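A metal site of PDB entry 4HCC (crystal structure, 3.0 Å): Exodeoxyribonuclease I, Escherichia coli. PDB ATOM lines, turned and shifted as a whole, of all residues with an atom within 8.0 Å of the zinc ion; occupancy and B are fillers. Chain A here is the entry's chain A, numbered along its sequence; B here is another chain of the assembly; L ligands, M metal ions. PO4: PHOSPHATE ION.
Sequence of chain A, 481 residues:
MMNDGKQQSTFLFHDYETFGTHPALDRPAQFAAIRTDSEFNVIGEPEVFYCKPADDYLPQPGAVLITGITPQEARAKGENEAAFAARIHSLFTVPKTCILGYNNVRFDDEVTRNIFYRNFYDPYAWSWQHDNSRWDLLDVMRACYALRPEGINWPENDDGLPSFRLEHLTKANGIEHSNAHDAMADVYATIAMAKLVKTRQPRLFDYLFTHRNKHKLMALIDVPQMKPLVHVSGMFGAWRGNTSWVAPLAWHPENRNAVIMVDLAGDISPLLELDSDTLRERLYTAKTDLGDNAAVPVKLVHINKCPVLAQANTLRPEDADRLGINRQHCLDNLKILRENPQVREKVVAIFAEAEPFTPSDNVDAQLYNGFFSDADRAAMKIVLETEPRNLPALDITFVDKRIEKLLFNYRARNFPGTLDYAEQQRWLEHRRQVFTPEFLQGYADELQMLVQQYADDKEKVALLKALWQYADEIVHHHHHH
O of Glu 17 sits at hydrogen-bond distance from N of Gln 30, at 2.9 Å. The side-chain carboxylate (OD1) of Asp 186 sits close to the backbone NH (N) of His 181 (3.3 Å). OG1 of Thr 190 sits at hydrogen-bond distance from O of Asp 186 (2.5 Å). The backbone NH (N) of Tyr 16 sits at hydrogen-bond distance from the side-chain carboxylate (OD1) of Asp 108 (3.0 Å).
Merely in contact with the zinc ion: Tyr 16 (3.97 Å). Within 4 Å of the zinc ion: Asp 15, Tyr 16, Glu 17 and Asp 186. The nearest printed residue that does not touch the zinc ion is DA 12 of chain B (4.02 Å).
The zinc ion is bound by an oxygen (O4) of the ligand (1.9 Å), the side-chain carboxylate of Asp 15 (2.0 Å), the side-chain carboxylate of Glu 17 (2.2 Å) and the side-chain carboxylate of Asp 186 (2.5 Å). The zinc ion has four donor atoms within binding distance.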
ATOM      1  N   HIS A  14       7.234  21.581   2.979  1.00  0.00           N
ATOM      2  CA  HIS A  14       6.649  20.285   2.663  1.00  0.00           C
ATOM      3  C   HIS A  14       6.806  19.290   3.769  1.00  0.00           C
ATOM      4  O   HIS A  14       7.657  19.451   4.661  1.00  0.00           O
ATOM      5  CB  HIS A  14       7.256  19.727   1.387  1.00  0.00           C
ATOM      6  CG  HIS A  14       8.645  19.195   1.557  1.00  0.00           C
ATOM      7  ND1 HIS A  14       9.730  19.990   1.596  1.00  0.00           N
ATOM      8  CD2 HIS A  14       9.108  17.891   1.706  1.00  0.00           C
ATOM      9  CE1 HIS A  14      10.833  19.234   1.772  1.00  0.00           C
ATOM     10  NE2 HIS A  14      10.456  17.953   1.830  1.00  0.00           N
ATOM     11  N   ASP A  15       5.974  18.247   3.719  1.00  0.00           N
ATOM     12  CA  ASP A  15       6.009  17.157   4.675  1.00  0.00           C
ATOM     13  C   ASP A  15       5.463  15.896   4.033  1.00  0.00           C
ATOM     14  O   ASP A  15       4.515  15.948   3.250  1.00  0.00           O
ATOM     15  CB  ASP A  15       5.168  17.494   5.894  1.00  0.00           C
ATOM     16  CG  ASP A  15       5.419  16.540   7.052  1.00  0.00           C
ATOM     17  OD1 ASP A  15       6.581  16.092   7.244  1.00  0.00           O
ATOM     18  OD2 ASP A  15       4.454  16.247   7.789  1.00  0.00           O
ATOM     19  N   TYR A  16       6.083  14.762   4.367  1.00  0.00           N
ATOM     20  CA  TYR A  16       5.562  13.461   4.016  1.00  0.00           C
ATOM     21  C   TYR A  16       5.016  12.751   5.254  1.00  0.00           C
ATOM     22  O   TYR A  16       5.499  12.970   6.362  1.00  0.00           O
ATOM     23  CB  TYR A  16       6.665  12.598   3.452  1.00  0.00           C
ATOM     24  CG  TYR A  16       7.175  12.964   2.079  1.00  0.00           C
ATOM     25  CD1 TYR A  16       6.609  12.398   0.928  1.00  0.00           C
ATOM     26  CD2 TYR A  16       8.244  13.840   1.918  1.00  0.00           C
ATOM     27  CE1 TYR A  16       7.098  12.722  -0.328  1.00  0.00           C
ATOM     28  CE2 TYR A  16       8.725  14.157   0.663  1.00  0.00           C
ATOM     29  CZ  TYR A  16       8.152  13.591  -0.455  1.00  0.00           C
ATOM     30  OH  TYR A  16       8.627  13.903  -1.699  1.00  0.00           O
ATOM     31  N   GLU A  17       4.007  11.909   5.054  1.00  0.00           N
ATOM     32  CA  GLU A  17       3.706  10.812   5.971  1.00  0.00           C
ATOM     33  C   GLU A  17       3.914   9.538   5.163  1.00  0.00           C
ATOM     34  O   GLU A  17       3.381   9.409   4.058  1.00  0.00           O
ATOM     35  CB  GLU A  17       2.283  10.893   6.503  1.00  0.00           C
ATOM     36  CG  GLU A  17       1.962  12.177   7.254  1.00  0.00           C
ATOM     37  CD  GLU A  17       2.959  12.509   8.344  1.00  0.00           C
ATOM     38  OE1 GLU A  17       3.266  11.617   9.174  1.00  0.00           O
ATOM     39  OE2 GLU A  17       3.443  13.659   8.392  1.00  0.00           O
ATOM     40  N   THR A  18       4.703   8.608   5.691  1.00  0.00           N
ATOM     41  CA  THR A  18       5.070   7.398   4.951  1.00  0.00           C
ATOM     42  C   THR A  18       4.606   6.133   5.654  1.00  0.00           C
ATOM     43  O   THR A  18       4.137   6.177   6.794  1.00  0.00           O
ATOM     44  CB  THR A  18       6.594   7.299   4.715  1.00  0.00           C
ATOM     45  OG1 THR A  18       7.253   6.955   5.943  1.00  0.00           O
ATOM     46  CG2 THR A  18       7.149   8.605   4.177  1.00  0.00           C
ATOM     47  N   GLN A  30       1.394  10.240   2.173  1.00  0.00           N
ATOM     48  CA  GLN A  30       0.785  11.556   2.078  1.00  0.00           C
ATOM     49  C   GLN A  30       1.861  12.588   1.828  1.00  0.00           C
ATOM     50  O   GLN A  30       2.996  12.431   2.280  1.00  0.00           O
ATOM     51  CB  GLN A  30       0.071  11.889   3.382  1.00  0.00           C
ATOM     52  CG  GLN A  30      -1.068  12.882   3.250  1.00  0.00           C
ATOM     53  CD  GLN A  30      -1.523  13.420   4.595  1.00  0.00           C
ATOM     54  OE1 GLN A  30      -0.854  13.233   5.610  1.00  0.00           O
ATOM     55  NE2 GLN A  30      -2.673  14.085   4.601  1.00  0.00           N
ATOM     56  N   ILE A  66       1.129   5.475  14.036  1.00  0.00           N
ATOM     57  CA  ILE A  66       1.500   6.868  14.238  1.00  0.00           C
ATOM     58  C   ILE A  66       0.671   7.854  13.413  1.00  0.00           C
ATOM     59  O   ILE A  66       0.236   8.880  13.947  1.00  0.00           O
ATOM     60  CB  ILE A  66       3.015   7.068  13.981  1.00  0.00           C
ATOM     61  CG1 ILE A  66       3.812   6.613  15.216  1.00  0.00           C
ATOM     62  CG2 ILE A  66       3.332   8.520  13.623  1.00  0.00           C
ATOM     63  CD1 ILE A  66       5.308   6.488  14.995  1.00  0.00           C
ATOM     64  N   THR A  67       0.428   7.538  12.147  1.00  0.00           N
ATOM     65  CA  THR A  67      -0.246   8.463  11.225  1.00  0.00           C
ATOM     66  C   THR A  67      -1.734   8.264  11.077  1.00  0.00           C
ATOM     67  O   THR A  67      -2.420   9.143  10.576  1.00  0.00           O
ATOM     68  CB  THR A  67       0.349   8.396   9.811  1.00  0.00           C
ATOM     69  OG1 THR A  67       0.056   7.106   9.236  1.00  0.00           O
ATOM     70  CG2 THR A  67       1.855   8.615   9.864  1.00  0.00           C
ATOM     71  N   TYR A 102      10.752  20.093   8.257  1.00  0.00           N
ATOM     72  CA  TYR A 102      11.227  19.771   9.598  1.00  0.00           C
ATOM     73  C   TYR A 102      11.816  18.358   9.634  1.00  0.00           C
ATOM     74  O   TYR A 102      11.091  17.371   9.490  1.00  0.00           O
ATOM     75  CB  TYR A 102      10.095  19.901  10.599  1.00  0.00           C
ATOM     76  CG  TYR A 102      10.549  20.205  12.003  1.00  0.00           C
ATOM     77  CD1 TYR A 102      11.067  21.457  12.323  1.00  0.00           C
ATOM     78  CD2 TYR A 102      10.419  19.257  13.010  1.00  0.00           C
ATOM     79  CE1 TYR A 102      11.459  21.746  13.617  1.00  0.00           C
ATOM     80  CE2 TYR A 102      10.818  19.538  14.302  1.00  0.00           C
ATOM     81  CZ  TYR A 102      11.337  20.783  14.601  1.00  0.00           C
ATOM     82  OH  TYR A 102      11.727  21.072  15.885  1.00  0.00           O
ATOM     83  N   PHE A 107      15.298  12.829   6.613  1.00  0.00           N
ATOM     84  CA  PHE A 107      14.167  11.985   6.256  1.00  0.00           C
ATOM     85  C   PHE A 107      13.537  12.362   4.920  1.00  0.00           C
ATOM     86  O   PHE A 107      13.722  11.688   3.918  1.00  0.00           O
ATOM     87  CB  PHE A 107      13.121  11.936   7.387  1.00  0.00           C
ATOM     88  CG  PHE A 107      12.009  10.954   7.134  1.00  0.00           C
ATOM     89  CD1 PHE A 107      12.261   9.578   7.112  1.00  0.00           C
ATOM     90  CD2 PHE A 107      10.714  11.393   6.899  1.00  0.00           C
ATOM     91  CE1 PHE A 107      11.245   8.673   6.871  1.00  0.00           C
ATOM     92  CE2 PHE A 107       9.684  10.489   6.661  1.00  0.00           C
ATOM     93  CZ  PHE A 107       9.953   9.125   6.646  1.00  0.00           C
ATOM     94  N   ASP A 108      12.821  13.474   4.883  1.00  0.00           N
ATOM     95  CA  ASP A 108      11.949  13.792   3.753  1.00  0.00           C
ATOM     96  C   ASP A 108      12.660  13.885   2.410  1.00  0.00           C
ATOM     97  O   ASP A 108      12.128  13.436   1.398  1.00  0.00           O
ATOM     98  CB  ASP A 108      11.105  15.039   4.065  1.00  0.00           C
ATOM     99  CG  ASP A 108      10.232  14.847   5.308  1.00  0.00           C
ATOM    100  OD1 ASP A 108       9.014  14.640   5.141  1.00  0.00           O
ATOM    101  OD2 ASP A 108      10.770  14.870   6.440  1.00  0.00           O
ATOM    102  N   LEU A 166       7.919  18.716  17.224  1.00  0.00           N
ATOM    103  CA  LEU A 166       7.174  19.862  16.713  1.00  0.00           C
ATOM    104  C   LEU A 166       5.907  20.162  17.503  1.00  0.00           C
ATOM    105  O   LEU A 166       5.591  21.315  17.779  1.00  0.00           O
ATOM    106  CB  LEU A 166       6.864  19.682  15.230  1.00  0.00           C
ATOM    107  CG  LEU A 166       6.242  20.862  14.478  1.00  0.00           C
ATOM    108  CD1 LEU A 166       7.085  22.124  14.593  1.00  0.00           C
ATOM    109  CD2 LEU A 166       6.032  20.467  13.028  1.00  0.00           C
ATOM    110  N   ASN A 179      -4.389  17.520  15.605  1.00  0.00           N
ATOM    111  CA  ASN A 179      -4.044  16.334  14.790  1.00  0.00           C
ATOM    112  C   ASN A 179      -2.658  16.343  14.125  1.00  0.00           C
ATOM    113  O   ASN A 179      -2.517  16.490  12.910  1.00  0.00           O
ATOM    114  CB  ASN A 179      -5.177  15.964  13.790  1.00  0.00           C
ATOM    115  CG  ASN A 179      -5.419  17.023  12.735  1.00  0.00           C
ATOM    116  OD1 ASN A 179      -6.006  18.071  13.006  1.00  0.00           O
ATOM    117  ND2 ASN A 179      -5.013  16.736  11.501  1.00  0.00           N
ATOM    118  N   ALA A 180      -1.642  16.149  14.972  1.00  0.00           N
ATOM    119  CA  ALA A 180      -0.252  16.049  14.529  1.00  0.00           C
ATOM    120  C   ALA A 180       0.015  14.749  13.768  1.00  0.00           C
ATOM    121  O   ALA A 180      -0.732  13.775  13.906  1.00  0.00           O
ATOM    122  CB  ALA A 180       0.686  16.179  15.719  1.00  0.00           C
ATOM    123  N   HIS A 181       1.083  14.757  12.979  1.00  0.00           N
ATOM    124  CA  HIS A 181       1.427  13.657  12.064  1.00  0.00           C
ATOM    125  C   HIS A 181       0.450  13.523  10.924  1.00  0.00           C
ATOM    126  O   HIS A 181       0.453  12.535  10.199  1.00  0.00           O
ATOM    127  CB  HIS A 181       1.673  12.359  12.835  1.00  0.00           C
ATOM    128  CG  HIS A 181       2.561  12.535  14.047  1.00  0.00           C
ATOM    129  ND1 HIS A 181       3.851  12.909  13.957  1.00  0.00           N
ATOM    130  CD2 HIS A 181       2.287  12.419  15.405  1.00  0.00           C
ATOM    131  CE1 HIS A 181       4.387  13.002  15.183  1.00  0.00           C
ATOM    132  NE2 HIS A 181       3.427  12.707  16.073  1.00  0.00           N
ATOM    133  N   ASP A 182      -0.400  14.533  10.780  1.00  0.00           N
ATOM    134  CA  ASP A 182      -1.049  14.827   9.518  1.00  0.00           C
ATOM    135  C   ASP A 182      -0.158  15.857   8.797  1.00  0.00           C
ATOM    136  O   ASP A 182       0.180  16.909   9.366  1.00  0.00           O
ATOM    137  CB  ASP A 182      -2.451  15.384   9.740  1.00  0.00           C
ATOM    138  CG  ASP A 182      -3.045  16.034   8.496  1.00  0.00           C
ATOM    139  OD1 ASP A 182      -3.078  15.379   7.420  1.00  0.00           O
ATOM    140  OD2 ASP A 182      -3.471  17.212   8.592  1.00  0.00           O
ATOM    141  N   ALA A 183       0.201  15.561   7.552  1.00  0.00           N
ATOM    142  CA  ALA A 183       1.163  16.380   6.798  1.00  0.00           C
ATOM    143  C   ALA A 183       0.847  17.883   6.776  1.00  0.00           C
ATOM    144  O   ALA A 183       1.674  18.703   7.180  1.00  0.00           O
ATOM    145  CB  ALA A 183       1.356  15.822   5.398  1.00  0.00           C
ATOM    146  N   MET A 184      -0.358  18.245   6.325  1.00  0.00           N
ATOM    147  CA  MET A 184      -0.778  19.651   6.231  1.00  0.00           C
ATOM    148  C   MET A 184      -0.617  20.414   7.548  1.00  0.00           C
ATOM    149  O   MET A 184      -0.120  21.542   7.562  1.00  0.00           O
ATOM    150  CB  MET A 184      -2.225  19.757   5.734  1.00  0.00           C
ATOM    151  CG  MET A 184      -2.685  21.162   5.362  1.00  0.00           C
ATOM    152  SD  MET A 184      -1.966  21.774   3.827  1.00  0.00           S
ATOM    153  CE  MET A 184      -0.433  22.455   4.419  1.00  0.00           C
ATOM    154  N   ALA A 185      -1.011  19.792   8.653  1.00  0.00           N
ATOM    155  CA  ALA A 185      -0.929  20.412   9.963  1.00  0.00           C
ATOM    156  C   ALA A 185       0.520  20.668  10.367  1.00  0.00           C
ATOM    157  O   ALA A 185       0.836  21.737  10.900  1.00  0.00           O
ATOM    158  CB  ALA A 185      -1.647  19.577  11.000  1.00  0.00           C
ATOM    159  N   ASP A 186       1.386  19.688  10.118  1.00  0.00           N
ATOM    160  CA  ASP A 186       2.811  19.820  10.463  1.00  0.00           C
ATOM    161  C   ASP A 186       3.523  20.895   9.639  1.00  0.00           C
ATOM    162  O   ASP A 186       4.361  21.621  10.160  1.00  0.00           O
ATOM    163  CB  ASP A 186       3.531  18.475  10.380  1.00  0.00           C
ATOM    164  CG  ASP A 186       3.219  17.561  11.571  1.00  0.00           C
ATOM    165  OD1 ASP A 186       3.591  16.380  11.528  1.00  0.00           O
ATOM    166  OD2 ASP A 186       2.600  18.038  12.561  1.00  0.00           O
ATOM    167  N   VAL A 187       3.154  21.015   8.361  1.00  0.00           N
ATOM    168  CA  VAL A 187       3.608  22.147   7.565  1.00  0.00           C
ATOM    169  C   VAL A 187       3.195  23.469   8.215  1.00  0.00           C
ATOM    170  O   VAL A 187       4.018  24.370   8.345  1.00  0.00           O
ATOM    171  CB  VAL A 187       3.085  22.084   6.121  1.00  0.00           C
ATOM    172  CG1 VAL A 187       3.251  23.417   5.425  1.00  0.00           C
ATOM    173  CG2 VAL A 187       3.800  21.001   5.329  1.00  0.00           C
ATOM    174  N   THR A 190       5.252  24.034  11.167  1.00  0.00           N
ATOM    175  CA  THR A 190       6.599  24.364  10.695  1.00  0.00           C
ATOM    176  C   THR A 190       6.669  25.837  10.330  1.00  0.00           C
ATOM    177  O   THR A 190       7.540  26.561  10.804  1.00  0.00           O
ATOM    178  CB  THR A 190       7.051  23.520   9.486  1.00  0.00           C
ATOM    179  OG1 THR A 190       6.799  22.141   9.749  1.00  0.00           O
ATOM    180  CG2 THR A 190       8.540  23.715   9.214  1.00  0.00           C
ATOM    181  P    DA B  12       9.532  15.209  15.430  1.00  0.00           P
ATOM    182  OP1  DA B  12       8.588  16.330  15.700  1.00  0.00           O
ATOM    183  OP2  DA B  12       9.393  13.937  16.194  1.00  0.00           O
ATOM    184  O5'  DA B  12       9.517  14.855  13.866  1.00  0.00           O
ATOM    185  C5'  DA B  12       9.173  13.532  13.435  1.00  0.00           C
ATOM    186  C4'  DA B  12       9.541  13.287  11.984  1.00  0.00           C
ATOM    187  O4'  DA B  12      10.899  12.781  11.906  1.00  0.00           O
ATOM    188  C3'  DA B  12       8.658  12.225  11.320  1.00  0.00           C
ATOM    189  O3'  DA B  12       7.661  12.835  10.502  1.00  0.00           O
ATOM    190  C2'  DA B  12       9.646  11.381  10.525  1.00  0.00           C
ATOM    191  C1'  DA B  12      10.891  11.467  11.380  1.00  0.00           C
ATOM    192  N9   DA B  12      10.952  10.522  12.498  1.00  0.00           N
ATOM    193  C8   DA B  12      10.460  10.716  13.770  1.00  0.00           C
ATOM    194  N7   DA B  12      10.662   9.691  14.568  1.00  0.00           N
ATOM    195  C5   DA B  12      11.340   8.775  13.778  1.00  0.00           C
ATOM    196  C6   DA B  12      11.844   7.494  14.041  1.00  0.00           C
ATOM    197  N6   DA B  12      11.738   6.883  15.226  1.00  0.00           N
ATOM    198  N1   DA B  12      12.467   6.840  13.036  1.00  0.00           N
ATOM    199  C2   DA B  12      12.581   7.458  11.849  1.00  0.00           C
ATOM    200  N3   DA B  12      12.140   8.656  11.478  1.00  0.00           N
ATOM    201  C4   DA B  12      11.525   9.274  12.501  1.00  0.00           C
HETATM  202  P   PO4 L   1       6.310  13.427  11.134  1.00  0.00           P
HETATM  203  O1  PO4 L   1       5.223  12.374  10.627  1.00  0.00           O
HETATM  204  O3  PO4 L   1       6.330  13.341  12.623  1.00  0.00           O
HETATM  205  O4  PO4 L   1       6.064  14.738  10.486  1.00  0.00           O
HETATM  206 ZN    ZN M   1       4.562  15.201   9.509  1.00  0.00          ZN
